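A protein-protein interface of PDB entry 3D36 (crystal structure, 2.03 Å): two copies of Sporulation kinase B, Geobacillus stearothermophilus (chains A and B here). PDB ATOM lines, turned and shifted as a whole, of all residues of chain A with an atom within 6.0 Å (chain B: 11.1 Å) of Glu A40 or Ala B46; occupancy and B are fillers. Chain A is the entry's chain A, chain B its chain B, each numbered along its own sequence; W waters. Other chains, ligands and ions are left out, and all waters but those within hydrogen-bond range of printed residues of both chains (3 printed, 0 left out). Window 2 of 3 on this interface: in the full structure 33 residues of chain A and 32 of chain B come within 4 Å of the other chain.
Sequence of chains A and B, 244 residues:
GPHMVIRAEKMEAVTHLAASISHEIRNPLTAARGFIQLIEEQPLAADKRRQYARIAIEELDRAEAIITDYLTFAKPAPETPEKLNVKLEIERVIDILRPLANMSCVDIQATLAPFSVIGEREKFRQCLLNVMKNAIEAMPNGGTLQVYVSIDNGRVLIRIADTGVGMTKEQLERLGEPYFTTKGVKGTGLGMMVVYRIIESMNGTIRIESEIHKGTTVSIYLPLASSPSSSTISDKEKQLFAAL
The side-chain carboxylate (OE1) of Glu A40 is in salt-bridge range of the guanidinium group (NE) of Arg B49 (2.9 Å). The guanidinium group (NE) of Arg B49 sits close to the guanidinium group (NE) of Arg A49, 3.4 Å away.
The guanidinium group of Arg A49 is in hydrogen-bond range of the backbone carbonyl oxygen of Gln A42. The guanidinium group (NH1) of Arg A49 is in hydrogen-bond range of the backbone carbonyl oxygen (O) of Pro A43, 3.1 Å away. O of Leu B44 sits at hydrogen-bond distance from NH1 of Arg B49 (2.8 Å).
CG1 of Ile A36 touches CD1 of Ile B36 (3.7 Å). Ile A36 touches Ala B53. Ile A36 touches Ile B57. Gln A37 touches Ile B57 (CG to CD1, 3.99 Å). Glu A40 touches Ala B46 (OE2 to O, 3.8 Å).
Of the printed residues of chain B, Gln A37 touches Ile B57 (3.99 Å). Leu A38 touches none of the printed residues of chain B. No residue of chain B comes within 4 Å of Ile A39. Glu A40 touches just these residues of chain B: Ala B46 (3.8 Å) and Arg B49 (2.9 Å). No residue of chain B comes within 4 Å of Pro A43. Of chain A, only Glu A40 (3.8 Å) comes within 4 Å of Ala B46. Asp B47 touches none of the printed residues of chain A. Of the printed residues of chain A, Ala B53 touches Ile A36 (3.7 Å). The nearest printed residue of chain A that does not touch Ala B46 is Pro A43 (6.5 Å).
Printed residues of chain A that touch a printed residue of chain B: Ile A36, Gln A37, Glu A40 and Arg A49. Hydrophobic or aromatic side chains of chain A that line the printed part of chain B: Ile A36. Of the 20 printed residues of chain B, 5 touch a printed residue of chain A. Hydrophobic or aromatic side chains of chain B within 4 Å of the printed part of chain A: Ile B36, Ala B53 and Ile B57. Along chain B the printed residues that touch a printed residue of chain A span positions 36 to 57.
Ile A36 touches its own counterpart, Ile B36. Glu A40 touches Arg B49, but with the chains exchanged Arg A49 does not touch Glu B40 (6.3 Å). Arg A49 touches its own counterpart, Arg B49. 8 positions are printed for both chains.
Water W3 lies within hydrogen-bond range of the backbone carbonyl oxygen (O) of Leu B44 (2.7 Å), the guanidinium group (NH2) of Arg A49 (3.0 Å) and the guanidinium group (NH1) of Arg B49 (3.2 Å). Water W2 lies within hydrogen-bond range of the backbone carbonyl oxygen (O) of Pro A43 (2.7 Å) and the guanidinium group (NH2) of Arg B49 (3.0 Å). Water W1 lies within hydrogen-bond range of the side-chain carboxylate of Glu A40 (2.8 Å) and the backbone carbonyl oxygen of Arg B49 (3.0 Å).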
ATOM      1  N   ILE A  36      19.942 -10.172   5.502  1.00  0.00           N
ATOM      2  CA  ILE A  36      19.531  -8.842   5.027  1.00  0.00           C
ATOM      3  C   ILE A  36      20.744  -8.054   4.522  1.00  0.00           C
ATOM      4  O   ILE A  36      20.710  -7.479   3.427  1.00  0.00           O
ATOM      5  CB  ILE A  36      18.777  -8.033   6.113  1.00  0.00           C
ATOM      6  CG1 ILE A  36      17.423  -8.682   6.417  1.00  0.00           C
ATOM      7  CG2 ILE A  36      18.582  -6.568   5.668  1.00  0.00           C
ATOM      8  CD1 ILE A  36      16.771  -8.178   7.717  1.00  0.00           C
ATOM      9  N   GLN A  37      21.815  -8.051   5.311  1.00  0.00           N
ATOM     10  CA  GLN A  37      23.036  -7.325   4.965  1.00  0.00           C
ATOM     11  C   GLN A  37      23.781  -7.925   3.765  1.00  0.00           C
ATOM     12  O   GLN A  37      24.511  -7.217   3.067  1.00  0.00           O
ATOM     13  CB  GLN A  37      23.954  -7.205   6.192  1.00  0.00           C
ATOM     14  CG  GLN A  37      23.447  -6.175   7.227  1.00  0.00           C
ATOM     15  CD  GLN A  37      24.233  -6.209   8.534  1.00  0.00           C
ATOM     16  OE1 GLN A  37      24.122  -7.156   9.317  1.00  0.00           O
ATOM     17  NE2 GLN A  37      25.047  -5.181   8.765  1.00  0.00           N
ATOM     18  N   LEU A  38      23.582  -9.219   3.516  1.00  0.00           N
ATOM     19  CA  LEU A  38      24.195  -9.882   2.365  1.00  0.00           C
ATOM     20  C   LEU A  38      23.501  -9.611   1.027  1.00  0.00           C
ATOM     21  O   LEU A  38      24.089  -9.845  -0.032  1.00  0.00           O
ATOM     22  CB  LEU A  38      24.310 -11.394   2.607  1.00  0.00           C
ATOM     23  CG  LEU A  38      25.394 -11.877   3.571  1.00  0.00           C
ATOM     24  CD1 LEU A  38      25.307 -13.392   3.734  1.00  0.00           C
ATOM     25  CD2 LEU A  38      26.780 -11.469   3.088  1.00  0.00           C
ATOM     26  N   ILE A  39      22.260  -9.134   1.064  1.00  0.00           N
ATOM     27  CA  ILE A  39      21.501  -8.856  -0.166  1.00  0.00           C
ATOM     28  C   ILE A  39      22.300  -7.977  -1.140  1.00  0.00           C
ATOM     29  O   ILE A  39      22.409  -8.287  -2.328  1.00  0.00           O
ATOM     30  CB  ILE A  39      20.107  -8.239   0.124  1.00  0.00           C
ATOM     31  CG1 ILE A  39      19.216  -9.253   0.859  1.00  0.00           C
ATOM     32  CG2 ILE A  39      19.416  -7.792  -1.185  1.00  0.00           C
ATOM     33  CD1 ILE A  39      17.966  -8.631   1.477  1.00  0.00           C
ATOM     34  N   GLU A  40      22.885  -6.897  -0.636  1.00  0.00           N
ATOM     35  CA  GLU A  40      23.627  -6.005  -1.526  1.00  0.00           C
ATOM     36  C   GLU A  40      24.977  -6.573  -1.970  1.00  0.00           C
ATOM     37  O   GLU A  40      25.676  -5.987  -2.793  1.00  0.00           O
ATOM     38  CB  GLU A  40      23.733  -4.603  -0.933  1.00  0.00           C
ATOM     39  CG  GLU A  40      22.389  -3.875  -0.982  1.00  0.00           C
ATOM     40  CD  GLU A  40      21.646  -4.092  -2.306  1.00  0.00           C
ATOM     41  OE1 GLU A  40      20.663  -4.872  -2.352  1.00  0.00           O
ATOM     42  OE2 GLU A  40      22.053  -3.470  -3.310  1.00  0.00           O
ATOM     43  N   GLU A  41      25.308  -7.747  -1.444  1.00  0.00           N
ATOM     44  CA  GLU A  41      26.523  -8.437  -1.825  1.00  0.00           C
ATOM     45  C   GLU A  41      26.292  -9.414  -2.991  1.00  0.00           C
ATOM     46  O   GLU A  41      27.214 -10.119  -3.424  1.00  0.00           O
ATOM     47  CB  GLU A  41      27.111  -9.126  -0.594  1.00  0.00           C
ATOM     48  CG  GLU A  41      28.600  -9.317  -0.667  1.00  0.00           C
ATOM     49  CD  GLU A  41      29.423  -8.101  -0.260  1.00  0.00           C
ATOM     50  OE1 GLU A  41      30.610  -8.331   0.036  1.00  0.00           O
ATOM     51  OE2 GLU A  41      28.918  -6.949  -0.241  1.00  0.00           O
ATOM     52  N   GLN A  42      25.068  -9.426  -3.522  1.00  0.00           N
ATOM     53  CA  GLN A  42      24.762 -10.151  -4.767  1.00  0.00           C
ATOM     54  C   GLN A  42      24.162  -9.226  -5.840  1.00  0.00           C
ATOM     55  O   GLN A  42      23.039  -9.453  -6.292  1.00  0.00           O
ATOM     56  CB  GLN A  42      23.809 -11.327  -4.489  1.00  0.00           C
ATOM     57  CG  GLN A  42      24.330 -12.382  -3.495  1.00  0.00           C
ATOM     58  CD  GLN A  42      25.421 -13.273  -4.064  1.00  0.00           C
ATOM     59  OE1 GLN A  42      25.764 -13.175  -5.233  1.00  0.00           O
ATOM     60  NE2 GLN A  42      25.964 -14.161  -3.227  1.00  0.00           N
ATOM     61  N   PRO A  43      24.910  -8.186  -6.268  1.00  0.00           N
ATOM     62  CA  PRO A  43      24.326  -7.182  -7.167  1.00  0.00           C
ATOM     63  C   PRO A  43      23.987  -7.676  -8.584  1.00  0.00           C
ATOM     64  O   PRO A  43      23.254  -7.000  -9.306  1.00  0.00           O
ATOM     65  CB  PRO A  43      25.413  -6.102  -7.228  1.00  0.00           C
ATOM     66  CG  PRO A  43      26.680  -6.823  -6.966  1.00  0.00           C
ATOM     67  CD  PRO A  43      26.321  -7.883  -5.960  1.00  0.00           C
ATOM     68  N   ARG A  49      19.736 -12.775  -4.234  1.00  0.00           N
ATOM     69  CA  ARG A  49      19.182 -11.704  -3.410  1.00  0.00           C
ATOM     70  C   ARG A  49      17.838 -12.132  -2.857  1.00  0.00           C
ATOM     71  O   ARG A  49      17.555 -11.913  -1.679  1.00  0.00           O
ATOM     72  CB  ARG A  49      19.000 -10.402  -4.208  1.00  0.00           C
ATOM     73  CG  ARG A  49      20.287  -9.739  -4.640  1.00  0.00           C
ATOM     74  CD  ARG A  49      20.066  -8.281  -5.025  1.00  0.00           C
ATOM     75  NE  ARG A  49      19.205  -8.094  -6.201  1.00  0.00           N
ATOM     76  CZ  ARG A  49      19.635  -8.075  -7.465  1.00  0.00           C
ATOM     77  NH1 ARG A  49      20.918  -8.257  -7.749  1.00  0.00           N
ATOM     78  NH2 ARG A  49      18.775  -7.877  -8.456  1.00  0.00           N
ATOM     79  N   TYR A  52      18.204 -14.830  -0.062  1.00  0.00           N
ATOM     80  CA  TYR A  52      18.599 -14.145   1.171  1.00  0.00           C
ATOM     81  C   TYR A  52      17.403 -13.491   1.856  1.00  0.00           C
ATOM     82  O   TYR A  52      17.238 -13.606   3.073  1.00  0.00           O
ATOM     83  CB  TYR A  52      19.649 -13.062   0.888  1.00  0.00           C
ATOM     84  CG  TYR A  52      21.048 -13.553   0.569  1.00  0.00           C
ATOM     85  CD1 TYR A  52      21.443 -14.864   0.849  1.00  0.00           C
ATOM     86  CD2 TYR A  52      21.990 -12.687   0.013  1.00  0.00           C
ATOM     87  CE1 TYR A  52      22.734 -15.303   0.562  1.00  0.00           C
ATOM     88  CE2 TYR A  52      23.274 -13.111  -0.274  1.00  0.00           C
ATOM     89  CZ  TYR A  52      23.646 -14.411   0.006  1.00  0.00           C
ATOM     90  OH  TYR A  52      24.924 -14.820  -0.272  1.00  0.00           O
ATOM     91  N   PHE B  35       9.692  -4.332   5.240  1.00  0.00           N
ATOM     92  CA  PHE B  35      10.705  -3.820   4.313  1.00  0.00           C
ATOM     93  C   PHE B  35      11.416  -4.908   3.509  1.00  0.00           C
ATOM     94  O   PHE B  35      11.711  -4.714   2.327  1.00  0.00           O
ATOM     95  CB  PHE B  35      11.715  -2.924   5.039  1.00  0.00           C
ATOM     96  CG  PHE B  35      11.237  -1.514   5.222  1.00  0.00           C
ATOM     97  CD1 PHE B  35      10.814  -1.062   6.468  1.00  0.00           C
ATOM     98  CD2 PHE B  35      11.197  -0.638   4.142  1.00  0.00           C
ATOM     99  CE1 PHE B  35      10.358   0.250   6.637  1.00  0.00           C
ATOM    100  CE2 PHE B  35      10.746   0.672   4.299  1.00  0.00           C
ATOM    101  CZ  PHE B  35      10.328   1.117   5.552  1.00  0.00           C
ATOM    102  N   ILE B  36      11.692  -6.046   4.141  1.00  0.00           N
ATOM    103  CA  ILE B  36      12.342  -7.159   3.429  1.00  0.00           C
ATOM    104  C   ILE B  36      11.358  -7.821   2.465  1.00  0.00           C
ATOM    105  O   ILE B  36      11.746  -8.270   1.375  1.00  0.00           O
ATOM    106  CB  ILE B  36      13.000  -8.186   4.406  1.00  0.00           C
ATOM    107  CG1 ILE B  36      14.001  -7.485   5.337  1.00  0.00           C
ATOM    108  CG2 ILE B  36      13.697  -9.328   3.635  1.00  0.00           C
ATOM    109  CD1 ILE B  36      15.008  -6.534   4.628  1.00  0.00           C
ATOM    110  N   LEU B  38       9.209  -6.242   0.748  1.00  0.00           N
ATOM    111  CA  LEU B  38       9.246  -5.389  -0.448  1.00  0.00           C
ATOM    112  C   LEU B  38      10.351  -5.824  -1.407  1.00  0.00           C
ATOM    113  O   LEU B  38      10.153  -5.849  -2.623  1.00  0.00           O
ATOM    114  CB  LEU B  38       9.425  -3.914  -0.074  1.00  0.00           C
ATOM    115  CG  LEU B  38       8.308  -3.238   0.727  1.00  0.00           C
ATOM    116  CD1 LEU B  38       8.751  -1.865   1.206  1.00  0.00           C
ATOM    117  CD2 LEU B  38       7.013  -3.141  -0.074  1.00  0.00           C
ATOM    118  N   ILE B  39      11.505  -6.173  -0.842  1.00  0.00           N
ATOM    119  CA  ILE B  39      12.652  -6.655  -1.608  1.00  0.00           C
ATOM    120  C   ILE B  39      12.374  -8.039  -2.205  1.00  0.00           C
ATOM    121  O   ILE B  39      12.746  -8.310  -3.345  1.00  0.00           O
ATOM    122  CB  ILE B  39      13.936  -6.686  -0.731  1.00  0.00           C
ATOM    123  CG1 ILE B  39      14.294  -5.271  -0.251  1.00  0.00           C
ATOM    124  CG2 ILE B  39      15.118  -7.307  -1.482  1.00  0.00           C
ATOM    125  CD1 ILE B  39      15.474  -5.225   0.716  1.00  0.00           C
ATOM    126  N   GLU B  40      11.708  -8.896  -1.433  1.00  0.00           N
ATOM    127  CA  GLU B  40      11.437 -10.275  -1.846  1.00  0.00           C
ATOM    128  C   GLU B  40      10.397 -10.384  -2.970  1.00  0.00           C
ATOM    129  O   GLU B  40      10.597 -11.128  -3.931  1.00  0.00           O
ATOM    130  CB  GLU B  40      10.997 -11.113  -0.633  1.00  0.00           C
ATOM    131  CG  GLU B  40      10.982 -12.633  -0.857  1.00  0.00           C
ATOM    132  CD  GLU B  40       9.730 -13.148  -1.562  1.00  0.00           C
ATOM    133  OE1 GLU B  40       9.807 -14.222  -2.197  1.00  0.00           O
ATOM    134  OE2 GLU B  40       8.667 -12.491  -1.488  1.00  0.00           O
ATOM    135  N   GLN B  42       9.182  -8.570  -5.445  1.00  0.00           N
ATOM    136  CA  GLN B  42       9.464  -8.154  -6.819  1.00  0.00           C
ATOM    137  C   GLN B  42      10.873  -7.572  -6.921  1.00  0.00           C
ATOM    138  O   GLN B  42      11.412  -7.101  -5.922  1.00  0.00           O
ATOM    139  CB  GLN B  42       8.419  -7.141  -7.313  1.00  0.00           C
ATOM    140  CG  GLN B  42       8.449  -5.793  -6.599  1.00  0.00           C
ATOM    141  CD  GLN B  42       7.425  -4.818  -7.145  1.00  0.00           C
ATOM    142  OE1 GLN B  42       7.246  -4.690  -8.361  1.00  0.00           O
ATOM    143  NE2 GLN B  42       6.747  -4.113  -6.245  1.00  0.00           N
ATOM    144  N   PRO B  43      11.484  -7.617  -8.123  1.00  0.00           N
ATOM    145  CA  PRO B  43      12.808  -7.008  -8.284  1.00  0.00           C
ATOM    146  C   PRO B  43      12.756  -5.482  -8.162  1.00  0.00           C
ATOM    147  O   PRO B  43      12.037  -4.818  -8.912  1.00  0.00           O
ATOM    148  CB  PRO B  43      13.228  -7.429  -9.704  1.00  0.00           C
ATOM    149  CG  PRO B  43      12.291  -8.532 -10.089  1.00  0.00           C
ATOM    150  CD  PRO B  43      11.014  -8.235  -9.375  1.00  0.00           C
ATOM    151  N   LEU B  44      13.500  -4.946  -7.200  1.00  0.00           N
ATOM    152  CA  LEU B  44      13.612  -3.503  -7.003  1.00  0.00           C
ATOM    153  C   LEU B  44      15.005  -3.046  -7.409  1.00  0.00           C
ATOM    154  O   LEU B  44      15.943  -3.846  -7.434  1.00  0.00           O
ATOM    155  CB  LEU B  44      13.350  -3.133  -5.534  1.00  0.00           C
ATOM    156  CG  LEU B  44      12.004  -3.484  -4.893  1.00  0.00           C
ATOM    157  CD1 LEU B  44      12.031  -3.168  -3.393  1.00  0.00           C
ATOM    158  CD2 LEU B  44      10.842  -2.765  -5.580  1.00  0.00           C
ATOM    159  N   ALA B  45      15.140  -1.761  -7.723  1.00  0.00           N
ATOM    160  CA  ALA B  45      16.441  -1.177  -8.048  1.00  0.00           C
ATOM    161  C   ALA B  45      17.343  -1.169  -6.815  1.00  0.00           C
ATOM    162  O   ALA B  45      16.858  -1.218  -5.686  1.00  0.00           O
ATOM    163  CB  ALA B  45      16.276   0.230  -8.596  1.00  0.00           C
ATOM    164  N   ALA B  46      18.654  -1.104  -7.041  1.00  0.00           N
ATOM    165  CA  ALA B  46      19.630  -1.249  -5.964  1.00  0.00           C
ATOM    166  C   ALA B  46      19.501  -0.184  -4.873  1.00  0.00           C
ATOM    167  O   ALA B  46      19.713  -0.488  -3.702  1.00  0.00           O
ATOM    168  CB  ALA B  46      21.050  -1.290  -6.523  1.00  0.00           C
ATOM    169  N   ASP B  47      19.143   1.047  -5.249  1.00  0.00           N
ATOM    170  CA  ASP B  47      19.013   2.137  -4.266  1.00  0.00           C
ATOM    171  C   ASP B  47      17.901   1.894  -3.243  1.00  0.00           C
ATOM    172  O   ASP B  47      18.075   2.151  -2.048  1.00  0.00           O
ATOM    173  CB  ASP B  47      18.865   3.513  -4.952  1.00  0.00           C
ATOM    174  CG  ASP B  47      17.608   3.627  -5.810  1.00  0.00           C
ATOM    175  OD1 ASP B  47      17.142   2.620  -6.389  1.00  0.00           O
ATOM    176  OD2 ASP B  47      17.082   4.750  -5.921  1.00  0.00           O
ATOM    177  N   LYS B  48      16.770   1.381  -3.717  1.00  0.00           N
ATOM    178  CA  LYS B  48      15.647   1.056  -2.850  1.00  0.00           C
ATOM    179  C   LYS B  48      15.924  -0.166  -1.973  1.00  0.00           C
ATOM    180  O   LYS B  48      15.584  -0.167  -0.793  1.00  0.00           O
ATOM    181  CB  LYS B  48      14.361   0.872  -3.665  1.00  0.00           C
ATOM    182  CG  LYS B  48      13.808   2.177  -4.264  1.00  0.00           C
ATOM    183  CD  LYS B  48      13.375   3.156  -3.165  1.00  0.00           C
ATOM    184  CE  LYS B  48      12.698   4.396  -3.743  1.00  0.00           C
ATOM    185  NZ  LYS B  48      13.673   5.321  -4.388  1.00  0.00           N
ATOM    186  N   ARG B  49      16.539  -1.198  -2.553  1.00  0.00           N
ATOM    187  CA  ARG B  49      16.933  -2.383  -1.789  1.00  0.00           C
ATOM    188  C   ARG B  49      17.851  -1.995  -0.635  1.00  0.00           C
ATOM    189  O   ARG B  49      17.672  -2.468   0.476  1.00  0.00           O
ATOM    190  CB  ARG B  49      17.654  -3.410  -2.662  1.00  0.00           C
ATOM    191  CG  ARG B  49      16.850  -3.946  -3.833  1.00  0.00           C
ATOM    192  CD  ARG B  49      17.470  -5.232  -4.371  1.00  0.00           C
ATOM    193  NE  ARG B  49      18.892  -5.105  -4.684  1.00  0.00           N
ATOM    194  CZ  ARG B  49      19.384  -4.888  -5.905  1.00  0.00           C
ATOM    195  NH1 ARG B  49      18.571  -4.732  -6.947  1.00  0.00           N
ATOM    196  NH2 ARG B  49      20.694  -4.807  -6.083  1.00  0.00           N
ATOM    197  N   ARG B  50      18.844  -1.155  -0.929  1.00  0.00           N
ATOM    198  CA  ARG B  50      19.809  -0.697   0.061  1.00  0.00           C
ATOM    199  C   ARG B  50      19.117   0.069   1.195  1.00  0.00           C
ATOM    200  O   ARG B  50      19.391  -0.165   2.377  1.00  0.00           O
ATOM    201  CB  ARG B  50      20.865   0.176  -0.624  1.00  0.00           C
ATOM    202  CG  ARG B  50      21.886   0.831   0.311  1.00  0.00           C
ATOM    203  CD  ARG B  50      23.188   1.163  -0.423  1.00  0.00           C
ATOM    204  NE  ARG B  50      22.951   1.825  -1.701  1.00  0.00           N
ATOM    205  CZ  ARG B  50      23.242   1.326  -2.900  1.00  0.00           C
ATOM    206  NH1 ARG B  50      23.819   0.137  -3.039  1.00  0.00           N
ATOM    207  NH2 ARG B  50      22.957   2.036  -3.972  1.00  0.00           N
ATOM    208  N   GLN B  51      18.219   0.980   0.824  1.00  0.00           N
ATOM    209  CA  GLN B  51      17.482   1.774   1.801  1.00  0.00           C
ATOM    210  C   GLN B  51      16.556   0.903   2.657  1.00  0.00           C
ATOM    211  O   GLN B  51      16.518   1.053   3.885  1.00  0.00           O
ATOM    212  CB  GLN B  51      16.682   2.889   1.114  1.00  0.00           C
ATOM    213  CG  GLN B  51      15.769   3.673   2.060  1.00  0.00           C
ATOM    214  CD  GLN B  51      15.056   4.820   1.369  1.00  0.00           C
ATOM    215  OE1 GLN B  51      14.616   4.696   0.229  1.00  0.00           O
ATOM    216  NE2 GLN B  51      14.933   5.937   2.061  1.00  0.00           N
ATOM    217  N   TYR B  52      15.820   0.000   2.012  1.00  0.00           N
ATOM    218  CA  TYR B  52      14.879  -0.850   2.733  1.00  0.00           C
ATOM    219  C   TYR B  52      15.595  -1.785   3.698  1.00  0.00           C
ATOM    220  O   TYR B  52      15.109  -2.024   4.804  1.00  0.00           O
ATOM    221  CB  TYR B  52      13.980  -1.639   1.785  1.00  0.00           C
ATOM    222  CG  TYR B  52      13.024  -0.803   0.950  1.00  0.00           C
ATOM    223  CD1 TYR B  52      12.314  -1.383  -0.103  1.00  0.00           C
ATOM    224  CD2 TYR B  52      12.843   0.561   1.192  1.00  0.00           C
ATOM    225  CE1 TYR B  52      11.436  -0.636  -0.878  1.00  0.00           C
ATOM    226  CE2 TYR B  52      11.961   1.326   0.413  1.00  0.00           C
ATOM    227  CZ  TYR B  52      11.264   0.713  -0.619  1.00  0.00           C
ATOM    228  OH  TYR B  52      10.393   1.440  -1.398  1.00  0.00           O
ATOM    229  N   ALA B  53      16.751  -2.297   3.273  1.00  0.00           N
ATOM    230  CA  ALA B  53      17.582  -3.152   4.118  1.00  0.00           C
ATOM    231  C   ALA B  53      18.126  -2.389   5.334  1.00  0.00           C
ATOM    232  O   ALA B  53      18.134  -2.919   6.440  1.00  0.00           O
ATOM    233  CB  ALA B  53      18.731  -3.772   3.301  1.00  0.00           C
ATOM    234  N   ARG B  54      18.564  -1.147   5.121  1.00  0.00           N
ATOM    235  CA  ARG B  54      19.089  -0.305   6.199  1.00  0.00           C
ATOM    236  C   ARG B  54      18.019  -0.029   7.268  1.00  0.00           C
ATOM    237  O   ARG B  54      18.290  -0.145   8.470  1.00  0.00           O
ATOM    238  CB  ARG B  54      19.653   1.014   5.636  1.00  0.00           C
ATOM    239  CG  ARG B  54      20.096   2.028   6.701  1.00  0.00           C
ATOM    240  CD  ARG B  54      20.725   3.282   6.074  1.00  0.00           C
ATOM    241  NE  ARG B  54      19.731   4.134   5.414  1.00  0.00           N
ATOM    242  CZ  ARG B  54      19.673   4.361   4.103  1.00  0.00           C
ATOM    243  NH1 ARG B  54      20.561   3.810   3.277  1.00  0.00           N
ATOM    244  NH2 ARG B  54      18.731   5.164   3.614  1.00  0.00           N
ATOM    245  N   ILE B  55      16.812   0.337   6.830  1.00  0.00           N
ATOM    246  CA  ILE B  55      15.705   0.597   7.762  1.00  0.00           C
ATOM    247  C   ILE B  55      15.333  -0.669   8.542  1.00  0.00           C
ATOM    248  O   ILE B  55      15.081  -0.612   9.758  1.00  0.00           O
ATOM    249  CB  ILE B  55      14.470   1.201   7.055  1.00  0.00           C
ATOM    250  CG1 ILE B  55      14.802   2.601   6.496  1.00  0.00           C
ATOM    251  CG2 ILE B  55      13.285   1.301   8.033  1.00  0.00           C
ATOM    252  CD1 ILE B  55      13.771   3.144   5.509  1.00  0.00           C
ATOM    253  N   ILE B  57      17.332  -3.146   9.292  1.00  0.00           N
ATOM    254  CA  ILE B  57      18.392  -3.399  10.271  1.00  0.00           C
ATOM    255  C   ILE B  57      18.272  -2.486  11.498  1.00  0.00           C
ATOM    256  O   ILE B  57      18.451  -2.940  12.629  1.00  0.00           O
ATOM    257  CB  ILE B  57      19.815  -3.305   9.640  1.00  0.00           C
ATOM    258  CG1 ILE B  57      20.014  -4.382   8.557  1.00  0.00           C
ATOM    259  CG2 ILE B  57      20.914  -3.406  10.708  1.00  0.00           C
ATOM    260  CD1 ILE B  57      19.922  -5.816   9.066  1.00  0.00           C
HETATM  261  O   HOH W   1      19.627  -4.765   0.206  1.00  0.00           O
HETATM  262  O   HOH W   2      21.978  -4.644  -8.797  1.00  0.00           O
HETATM  263  O   HOH W   3      16.211  -6.373  -8.367  1.00  0.00           O
